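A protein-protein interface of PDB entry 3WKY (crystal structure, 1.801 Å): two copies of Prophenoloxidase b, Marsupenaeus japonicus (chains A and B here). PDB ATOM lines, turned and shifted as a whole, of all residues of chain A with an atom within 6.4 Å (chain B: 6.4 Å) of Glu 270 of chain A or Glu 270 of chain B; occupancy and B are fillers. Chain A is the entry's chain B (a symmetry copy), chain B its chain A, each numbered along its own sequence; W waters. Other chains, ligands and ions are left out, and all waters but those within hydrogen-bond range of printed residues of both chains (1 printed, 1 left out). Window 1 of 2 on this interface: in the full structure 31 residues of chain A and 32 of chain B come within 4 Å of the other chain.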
ATOM      1  N   THR A 145     -22.610  16.120  23.900  1.00  0.00           N
ATOM      2  CA  THR A 145     -23.256  15.058  24.659  1.00  0.00           C
ATOM      3  C   THR A 145     -22.254  14.265  25.490  1.00  0.00           C
ATOM      4  O   THR A 145     -22.453  14.054  26.692  1.00  0.00           O
ATOM      5  CB  THR A 145     -23.942  14.095  23.693  1.00  0.00           C
ATOM      6  OG1 THR A 145     -24.957  14.797  22.960  1.00  0.00           O
ATOM      7  CG2 THR A 145     -24.573  12.897  24.439  1.00  0.00           C
ATOM      8  N   HIS A 262     -23.978  16.642  17.823  1.00  0.00           N
ATOM      9  CA  HIS A 262     -23.525  15.986  19.061  1.00  0.00           C
ATOM     10  C   HIS A 262     -23.998  16.729  20.310  1.00  0.00           C
ATOM     11  O   HIS A 262     -23.203  17.001  21.214  1.00  0.00           O
ATOM     12  CB  HIS A 262     -21.997  15.829  19.066  1.00  0.00           C
ATOM     13  CG  HIS A 262     -21.491  14.898  18.005  1.00  0.00           C
ATOM     14  ND1 HIS A 262     -21.194  15.315  16.727  1.00  0.00           N
ATOM     15  CD2 HIS A 262     -21.259  13.564  18.030  1.00  0.00           C
ATOM     16  CE1 HIS A 262     -20.783  14.281  16.013  1.00  0.00           C
ATOM     17  NE2 HIS A 262     -20.812  13.209  16.781  1.00  0.00           N
ATOM     18  N   LEU A 263     -25.285  17.070  20.334  1.00  0.00           N
ATOM     19  CA  LEU A 263     -25.903  17.761  21.474  1.00  0.00           C
ATOM     20  C   LEU A 263     -27.127  17.011  21.973  1.00  0.00           C
ATOM     21  O   LEU A 263     -27.891  16.462  21.180  1.00  0.00           O
ATOM     22  CB  LEU A 263     -26.337  19.178  21.088  1.00  0.00           C
ATOM     23  CG  LEU A 263     -25.251  20.179  20.698  1.00  0.00           C
ATOM     24  CD1 LEU A 263     -25.918  21.496  20.299  1.00  0.00           C
ATOM     25  CD2 LEU A 263     -24.260  20.407  21.835  1.00  0.00           C
ATOM     26  N   THR A 264     -27.336  17.025  23.289  1.00  0.00           N
ATOM     27  CA  THR A 264     -28.501  16.382  23.899  1.00  0.00           C
ATOM     28  C   THR A 264     -29.096  17.334  24.932  1.00  0.00           C
ATOM     29  O   THR A 264     -28.359  17.877  25.758  1.00  0.00           O
ATOM     30  CB  THR A 264     -28.083  15.077  24.596  1.00  0.00           C
ATOM     31  OG1 THR A 264     -27.446  14.211  23.642  1.00  0.00           O
ATOM     32  CG2 THR A 264     -29.293  14.368  25.202  1.00  0.00           C
ATOM     33  N   THR A 265     -30.408  17.557  24.891  1.00  0.00           N
ATOM     34  CA  THR A 265     -31.017  18.498  25.844  1.00  0.00           C
ATOM     35  C   THR A 265     -31.073  17.887  27.239  1.00  0.00           C
ATOM     36  O   THR A 265     -30.894  16.677  27.403  1.00  0.00           O
ATOM     37  CB  THR A 265     -32.444  18.906  25.463  1.00  0.00           C
ATOM     38  OG1 THR A 265     -33.344  17.815  25.711  1.00  0.00           O
ATOM     39  CG2 THR A 265     -32.522  19.325  23.999  1.00  0.00           C
ATOM     40  N   GLY A 268     -32.888  14.824  27.979  1.00  0.00           N
ATOM     41  CA  GLY A 268     -32.383  13.584  27.402  1.00  0.00           C
ATOM     42  C   GLY A 268     -32.687  13.429  25.923  1.00  0.00           C
ATOM     43  O   GLY A 268     -32.422  12.374  25.332  1.00  0.00           O
ATOM     44  N   GLN A 269     -33.232  14.483  25.317  1.00  0.00           N
ATOM     45  CA  GLN A 269     -33.578  14.441  23.905  1.00  0.00           C
ATOM     46  C   GLN A 269     -32.403  14.902  23.027  1.00  0.00           C
ATOM     47  O   GLN A 269     -32.064  16.086  22.996  1.00  0.00           O
ATOM     48  CB  GLN A 269     -34.835  15.277  23.652  1.00  0.00           C
ATOM     49  CG  GLN A 269     -36.083  14.758  24.376  1.00  0.00           C
ATOM     50  CD  GLN A 269     -36.879  13.754  23.549  1.00  0.00           C
ATOM     51  OE1 GLN A 269     -36.765  12.541  23.737  1.00  0.00           O
ATOM     52  NE2 GLN A 269     -37.699  14.263  22.637  1.00  0.00           N
ATOM     53  N   GLU A 270     -31.780  13.952  22.329  1.00  0.00           N
ATOM     54  CA  GLU A 270     -30.661  14.255  21.437  1.00  0.00           C
ATOM     55  C   GLU A 270     -31.142  14.984  20.181  1.00  0.00           C
ATOM     56  O   GLU A 270     -32.114  14.549  19.559  1.00  0.00           O
ATOM     57  CB  GLU A 270     -29.927  12.972  21.034  1.00  0.00           C
ATOM     58  CG  GLU A 270     -28.836  13.218  19.979  1.00  0.00           C
ATOM     59  CD  GLU A 270     -27.864  12.061  19.799  1.00  0.00           C
ATOM     60  OE1 GLU A 270     -27.269  11.617  20.806  1.00  0.00           O
ATOM     61  OE2 GLU A 270     -27.685  11.605  18.643  1.00  0.00           O
ATOM     62  N   TRP A 271     -30.470  16.080  19.812  1.00  0.00           N
ATOM     63  CA  TRP A 271     -30.848  16.851  18.635  1.00  0.00           C
ATOM     64  C   TRP A 271     -30.640  16.004  17.380  1.00  0.00           C
ATOM     65  O   TRP A 271     -29.628  15.308  17.247  1.00  0.00           O
ATOM     66  CB  TRP A 271     -29.996  18.128  18.499  1.00  0.00           C
ATOM     67  CG  TRP A 271     -30.285  19.170  19.559  1.00  0.00           C
ATOM     68  CD1 TRP A 271     -29.817  19.184  20.844  1.00  0.00           C
ATOM     69  CD2 TRP A 271     -31.106  20.341  19.418  1.00  0.00           C
ATOM     70  NE1 TRP A 271     -30.304  20.284  21.510  1.00  0.00           N
ATOM     71  CE2 TRP A 271     -31.095  21.011  20.661  1.00  0.00           C
ATOM     72  CE3 TRP A 271     -31.845  20.888  18.363  1.00  0.00           C
ATOM     73  CZ2 TRP A 271     -31.795  22.202  20.873  1.00  0.00           C
ATOM     74  CZ3 TRP A 271     -32.553  22.059  18.583  1.00  0.00           C
ATOM     75  CH2 TRP A 271     -32.522  22.706  19.829  1.00  0.00           C
ATOM     76  N   SER A 272     -31.580  16.099  16.452  1.00  0.00           N
ATOM     77  CA  SER A 272     -31.458  15.403  15.178  1.00  0.00           C
ATOM     78  C   SER A 272     -30.273  15.933  14.387  1.00  0.00           C
ATOM     79  O   SER A 272     -29.872  17.090  14.541  1.00  0.00           O
ATOM     80  CB  SER A 272     -32.737  15.572  14.365  1.00  0.00           C
ATOM     81  OG  SER A 272     -33.804  14.889  15.007  1.00  0.00           O
ATOM     82  N   SER A 273     -29.712  15.068  13.554  1.00  0.00           N
ATOM     83  CA  SER A 273     -28.611  15.432  12.676  1.00  0.00           C
ATOM     84  C   SER A 273     -29.125  15.528  11.233  1.00  0.00           C
ATOM     85  O   SER A 273     -30.293  15.247  10.949  1.00  0.00           O
ATOM     86  CB  SER A 273     -27.503  14.385  12.757  1.00  0.00           C
ATOM     87  OG  SER A 273     -26.989  14.239  14.079  1.00  0.00           O
ATOM     88  N   THR A 377     -37.014  14.483  16.591  1.00  0.00           N
ATOM     89  CA  THR A 377     -36.792  15.828  17.075  1.00  0.00           C
ATOM     90  C   THR A 377     -36.274  16.723  15.927  1.00  0.00           C
ATOM     91  O   THR A 377     -35.954  16.234  14.853  1.00  0.00           O
ATOM     92  CB  THR A 377     -35.745  15.761  18.212  1.00  0.00           C
ATOM     93  OG1 THR A 377     -34.561  15.095  17.740  1.00  0.00           O
ATOM     94  CG2 THR A 377     -36.282  14.976  19.403  1.00  0.00           C
ATOM     95  N   SER A 378     -36.193  18.029  16.150  1.00  0.00           N
ATOM     96  CA  SER A 378     -35.681  18.941  15.124  1.00  0.00           C
ATOM     97  C   SER A 378     -34.152  19.029  15.158  1.00  0.00           C
ATOM     98  O   SER A 378     -33.520  18.680  16.160  1.00  0.00           O
ATOM     99  CB  SER A 378     -36.287  20.329  15.308  1.00  0.00           C
ATOM    100  OG  SER A 378     -35.575  21.315  14.573  1.00  0.00           O
ATOM    101  N   THR B 145     -34.939   5.092  24.140  1.00  0.00           N
ATOM    102  CA  THR B 145     -34.239   6.104  24.915  1.00  0.00           C
ATOM    103  C   THR B 145     -35.148   6.822  25.906  1.00  0.00           C
ATOM    104  O   THR B 145     -34.822   6.932  27.093  1.00  0.00           O
ATOM    105  CB  THR B 145     -33.653   7.147  23.967  1.00  0.00           C
ATOM    106  OG1 THR B 145     -32.728   6.509  23.070  1.00  0.00           O
ATOM    107  CG2 THR B 145     -32.947   8.257  24.747  1.00  0.00           C
ATOM    108  N   HIS B 262     -34.237   5.042  17.940  1.00  0.00           N
ATOM    109  CA  HIS B 262     -34.555   5.599  19.261  1.00  0.00           C
ATOM    110  C   HIS B 262     -33.948   4.767  20.396  1.00  0.00           C
ATOM    111  O   HIS B 262     -34.629   4.438  21.366  1.00  0.00           O
ATOM    112  CB  HIS B 262     -36.072   5.760  19.431  1.00  0.00           C
ATOM    113  CG  HIS B 262     -36.676   6.771  18.502  1.00  0.00           C
ATOM    114  ND1 HIS B 262     -37.117   6.451  17.236  1.00  0.00           N
ATOM    115  CD2 HIS B 262     -36.888   8.100  18.648  1.00  0.00           C
ATOM    116  CE1 HIS B 262     -37.585   7.539  16.647  1.00  0.00           C
ATOM    117  NE2 HIS B 262     -37.463   8.550  17.484  1.00  0.00           N
ATOM    118  N   LEU B 263     -32.669   4.428  20.254  1.00  0.00           N
ATOM    119  CA  LEU B 263     -31.934   3.647  21.258  1.00  0.00           C
ATOM    120  C   LEU B 263     -30.662   4.368  21.674  1.00  0.00           C
ATOM    121  O   LEU B 263     -29.996   4.986  20.840  1.00  0.00           O
ATOM    122  CB  LEU B 263     -31.542   2.277  20.701  1.00  0.00           C
ATOM    123  CG  LEU B 263     -32.669   1.304  20.340  1.00  0.00           C
ATOM    124  CD1 LEU B 263     -32.074   0.037  19.740  1.00  0.00           C
ATOM    125  CD2 LEU B 263     -33.535   0.969  21.556  1.00  0.00           C
ATOM    126  N   THR B 264     -30.307   4.259  22.955  1.00  0.00           N
ATOM    127  CA  THR B 264     -29.081   4.857  23.483  1.00  0.00           C
ATOM    128  C   THR B 264     -28.392   3.826  24.371  1.00  0.00           C
ATOM    129  O   THR B 264     -29.048   3.222  25.228  1.00  0.00           O
ATOM    130  CB  THR B 264     -29.401   6.105  24.325  1.00  0.00           C
ATOM    131  OG1 THR B 264     -30.140   7.046  23.526  1.00  0.00           O
ATOM    132  CG2 THR B 264     -28.122   6.768  24.848  1.00  0.00           C
ATOM    133  N   THR B 265     -27.093   3.608  24.173  1.00  0.00           N
ATOM    134  CA  THR B 265     -26.386   2.592  24.975  1.00  0.00           C
ATOM    135  C   THR B 265     -26.162   3.088  26.398  1.00  0.00           C
ATOM    136  O   THR B 265     -26.362   4.267  26.686  1.00  0.00           O
ATOM    137  CB  THR B 265     -25.010   2.210  24.402  1.00  0.00           C
ATOM    138  OG1 THR B 265     -24.078   3.287  24.603  1.00  0.00           O
ATOM    139  CG2 THR B 265     -25.102   1.864  22.920  1.00  0.00           C
ATOM    140  N   GLY B 268     -24.242   6.113  27.179  1.00  0.00           N
ATOM    141  CA  GLY B 268     -24.817   7.393  26.776  1.00  0.00           C
ATOM    142  C   GLY B 268     -24.729   7.667  25.286  1.00  0.00           C
ATOM    143  O   GLY B 268     -25.055   8.766  24.813  1.00  0.00           O
ATOM    144  N   GLN B 269     -24.296   6.653  24.543  1.00  0.00           N
ATOM    145  CA  GLN B 269     -24.104   6.768  23.104  1.00  0.00           C
ATOM    146  C   GLN B 269     -25.374   6.407  22.324  1.00  0.00           C
ATOM    147  O   GLN B 269     -25.719   5.227  22.222  1.00  0.00           O
ATOM    148  CB  GLN B 269     -22.963   5.844  22.688  1.00  0.00           C
ATOM    149  CG  GLN B 269     -21.622   6.220  23.285  1.00  0.00           C
ATOM    150  CD  GLN B 269     -20.698   6.858  22.262  1.00  0.00           C
ATOM    151  OE1 GLN B 269     -20.146   6.172  21.396  1.00  0.00           O
ATOM    152  NE2 GLN B 269     -20.530   8.178  22.351  1.00  0.00           N
ATOM    153  N   GLU B 270     -26.057   7.415  21.776  1.00  0.00           N
ATOM    154  CA  GLU B 270     -27.258   7.178  20.970  1.00  0.00           C
ATOM    155  C   GLU B 270     -26.909   6.563  19.613  1.00  0.00           C
ATOM    156  O   GLU B 270     -26.013   7.058  18.932  1.00  0.00           O
ATOM    157  CB  GLU B 270     -28.033   8.480  20.755  1.00  0.00           C
ATOM    158  CG  GLU B 270     -29.180   8.323  19.758  1.00  0.00           C
ATOM    159  CD  GLU B 270     -30.167   9.476  19.759  1.00  0.00           C
ATOM    160  OE1 GLU B 270     -30.416  10.042  18.667  1.00  0.00           O
ATOM    161  OE2 GLU B 270     -30.711   9.800  20.838  1.00  0.00           O
ATOM    162  N   TRP B 271     -27.605   5.488  19.229  1.00  0.00           N
ATOM    163  CA  TRP B 271     -27.335   4.819  17.967  1.00  0.00           C
ATOM    164  C   TRP B 271     -27.659   5.761  16.812  1.00  0.00           C
ATOM    165  O   TRP B 271     -28.666   6.479  16.837  1.00  0.00           O
ATOM    166  CB  TRP B 271     -28.191   3.549  17.817  1.00  0.00           C
ATOM    167  CG  TRP B 271     -27.797   2.430  18.757  1.00  0.00           C
ATOM    168  CD1 TRP B 271     -28.122   2.316  20.082  1.00  0.00           C
ATOM    169  CD2 TRP B 271     -27.009   1.270  18.435  1.00  0.00           C
ATOM    170  NE1 TRP B 271     -27.573   1.166  20.604  1.00  0.00           N
ATOM    171  CE2 TRP B 271     -26.894   0.502  19.616  1.00  0.00           C
ATOM    172  CE3 TRP B 271     -26.398   0.805  17.263  1.00  0.00           C
ATOM    173  CZ2 TRP B 271     -26.184  -0.701  19.658  1.00  0.00           C
ATOM    174  CZ3 TRP B 271     -25.686  -0.380  17.309  1.00  0.00           C
ATOM    175  CH2 TRP B 271     -25.586  -1.124  18.502  1.00  0.00           C
ATOM    176  N   SER B 272     -26.822   5.721  15.786  1.00  0.00           N
ATOM    177  CA  SER B 272     -27.064   6.500  14.580  1.00  0.00           C
ATOM    178  C   SER B 272     -28.342   6.039  13.894  1.00  0.00           C
ATOM    179  O   SER B 272     -28.749   4.880  14.018  1.00  0.00           O
ATOM    180  CB  SER B 272     -25.879   6.373  13.630  1.00  0.00           C
ATOM    181  OG  SER B 272     -24.747   7.014  14.202  1.00  0.00           O
ATOM    182  N   SER B 273     -28.975   6.963  13.183  1.00  0.00           N
ATOM    183  CA  SER B 273     -30.178   6.662  12.417  1.00  0.00           C
ATOM    184  C   SER B 273     -29.828   6.688  10.931  1.00  0.00           C
ATOM    185  O   SER B 273     -28.694   6.994  10.552  1.00  0.00           O
ATOM    186  CB  SER B 273     -31.249   7.710  12.705  1.00  0.00           C
ATOM    187  OG  SER B 273     -31.603   7.729  14.082  1.00  0.00           O
ATOM    188  N   THR B 377     -21.487   7.364  15.521  1.00  0.00           N
ATOM    189  CA  THR B 377     -21.718   5.980  15.901  1.00  0.00           C
ATOM    190  C   THR B 377     -22.257   5.160  14.709  1.00  0.00           C
ATOM    191  O   THR B 377     -22.612   5.716  13.679  1.00  0.00           O
ATOM    192  CB  THR B 377     -22.745   5.934  17.073  1.00  0.00           C
ATOM    193  OG1 THR B 377     -23.896   6.730  16.740  1.00  0.00           O
ATOM    194  CG2 THR B 377     -22.139   6.504  18.347  1.00  0.00           C
ATOM    195  N   SER B 378     -22.312   3.842  14.843  1.00  0.00           N
ATOM    196  CA  SER B 378     -22.907   3.000  13.803  1.00  0.00           C
ATOM    197  C   SER B 378     -24.421   2.899  13.992  1.00  0.00           C
ATOM    198  O   SER B 378     -24.943   3.162  15.082  1.00  0.00           O
ATOM    199  CB  SER B 378     -22.285   1.607  13.829  1.00  0.00           C
ATOM    200  OG  SER B 378     -23.070   0.668  13.101  1.00  0.00           O
HETATM  201  O   HOH W   1     -24.836   9.828  21.998  1.00  0.00           O
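OE2 of Glu 270 of chain A sits close to OE1 of Glu 270 of chain B, 3.1 Å away.
The backbone carbonyl oxygen (O) of Glu 270 of chain A lies within hydrogen-bond range of the side-chain hydroxyl (OG1) of Thr 377 of chain A (3.1 Å). The backbone carbonyl oxygen (O) of Glu 270 of chain B is in hydrogen-bond range of the side-chain hydroxyl (OG1) of Thr 377 of chain B.
Glu 270 of chain A touches one residue of chain B. Printed residues of chain A within 4 Å of Glu 270 of chain B: Glu 270. Ser 378 of chain B touches none of the printed residues of chain A. Leu 263 of chain B touches none of the printed residues of chain A. The nearest residue of chain B that does not touch Glu 270 of chain A is Gly 268 of chain B (5.4 Å). The nearest residue of chain A that does not touch Glu 270 of chain B is Gly 268 of chain A (5.5 Å).
Of the 13 printed residues of chain A, 1 touches a printed residue of chain B. Among the printed residues, no Asp or Glu carboxylate lies within 4 Å of a Lys or Arg side-chain nitrogen of the other chain.
Glu 270 of chain A touches its own counterpart, Glu 270 of chain B.
Water W1 lies within hydrogen-bond range of N of Glu 270 of chain B (2.7 Å), O of Gly 268 of chain B (3.0 Å) and OE1 of Glu 270 of chain A (3.2 Å).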
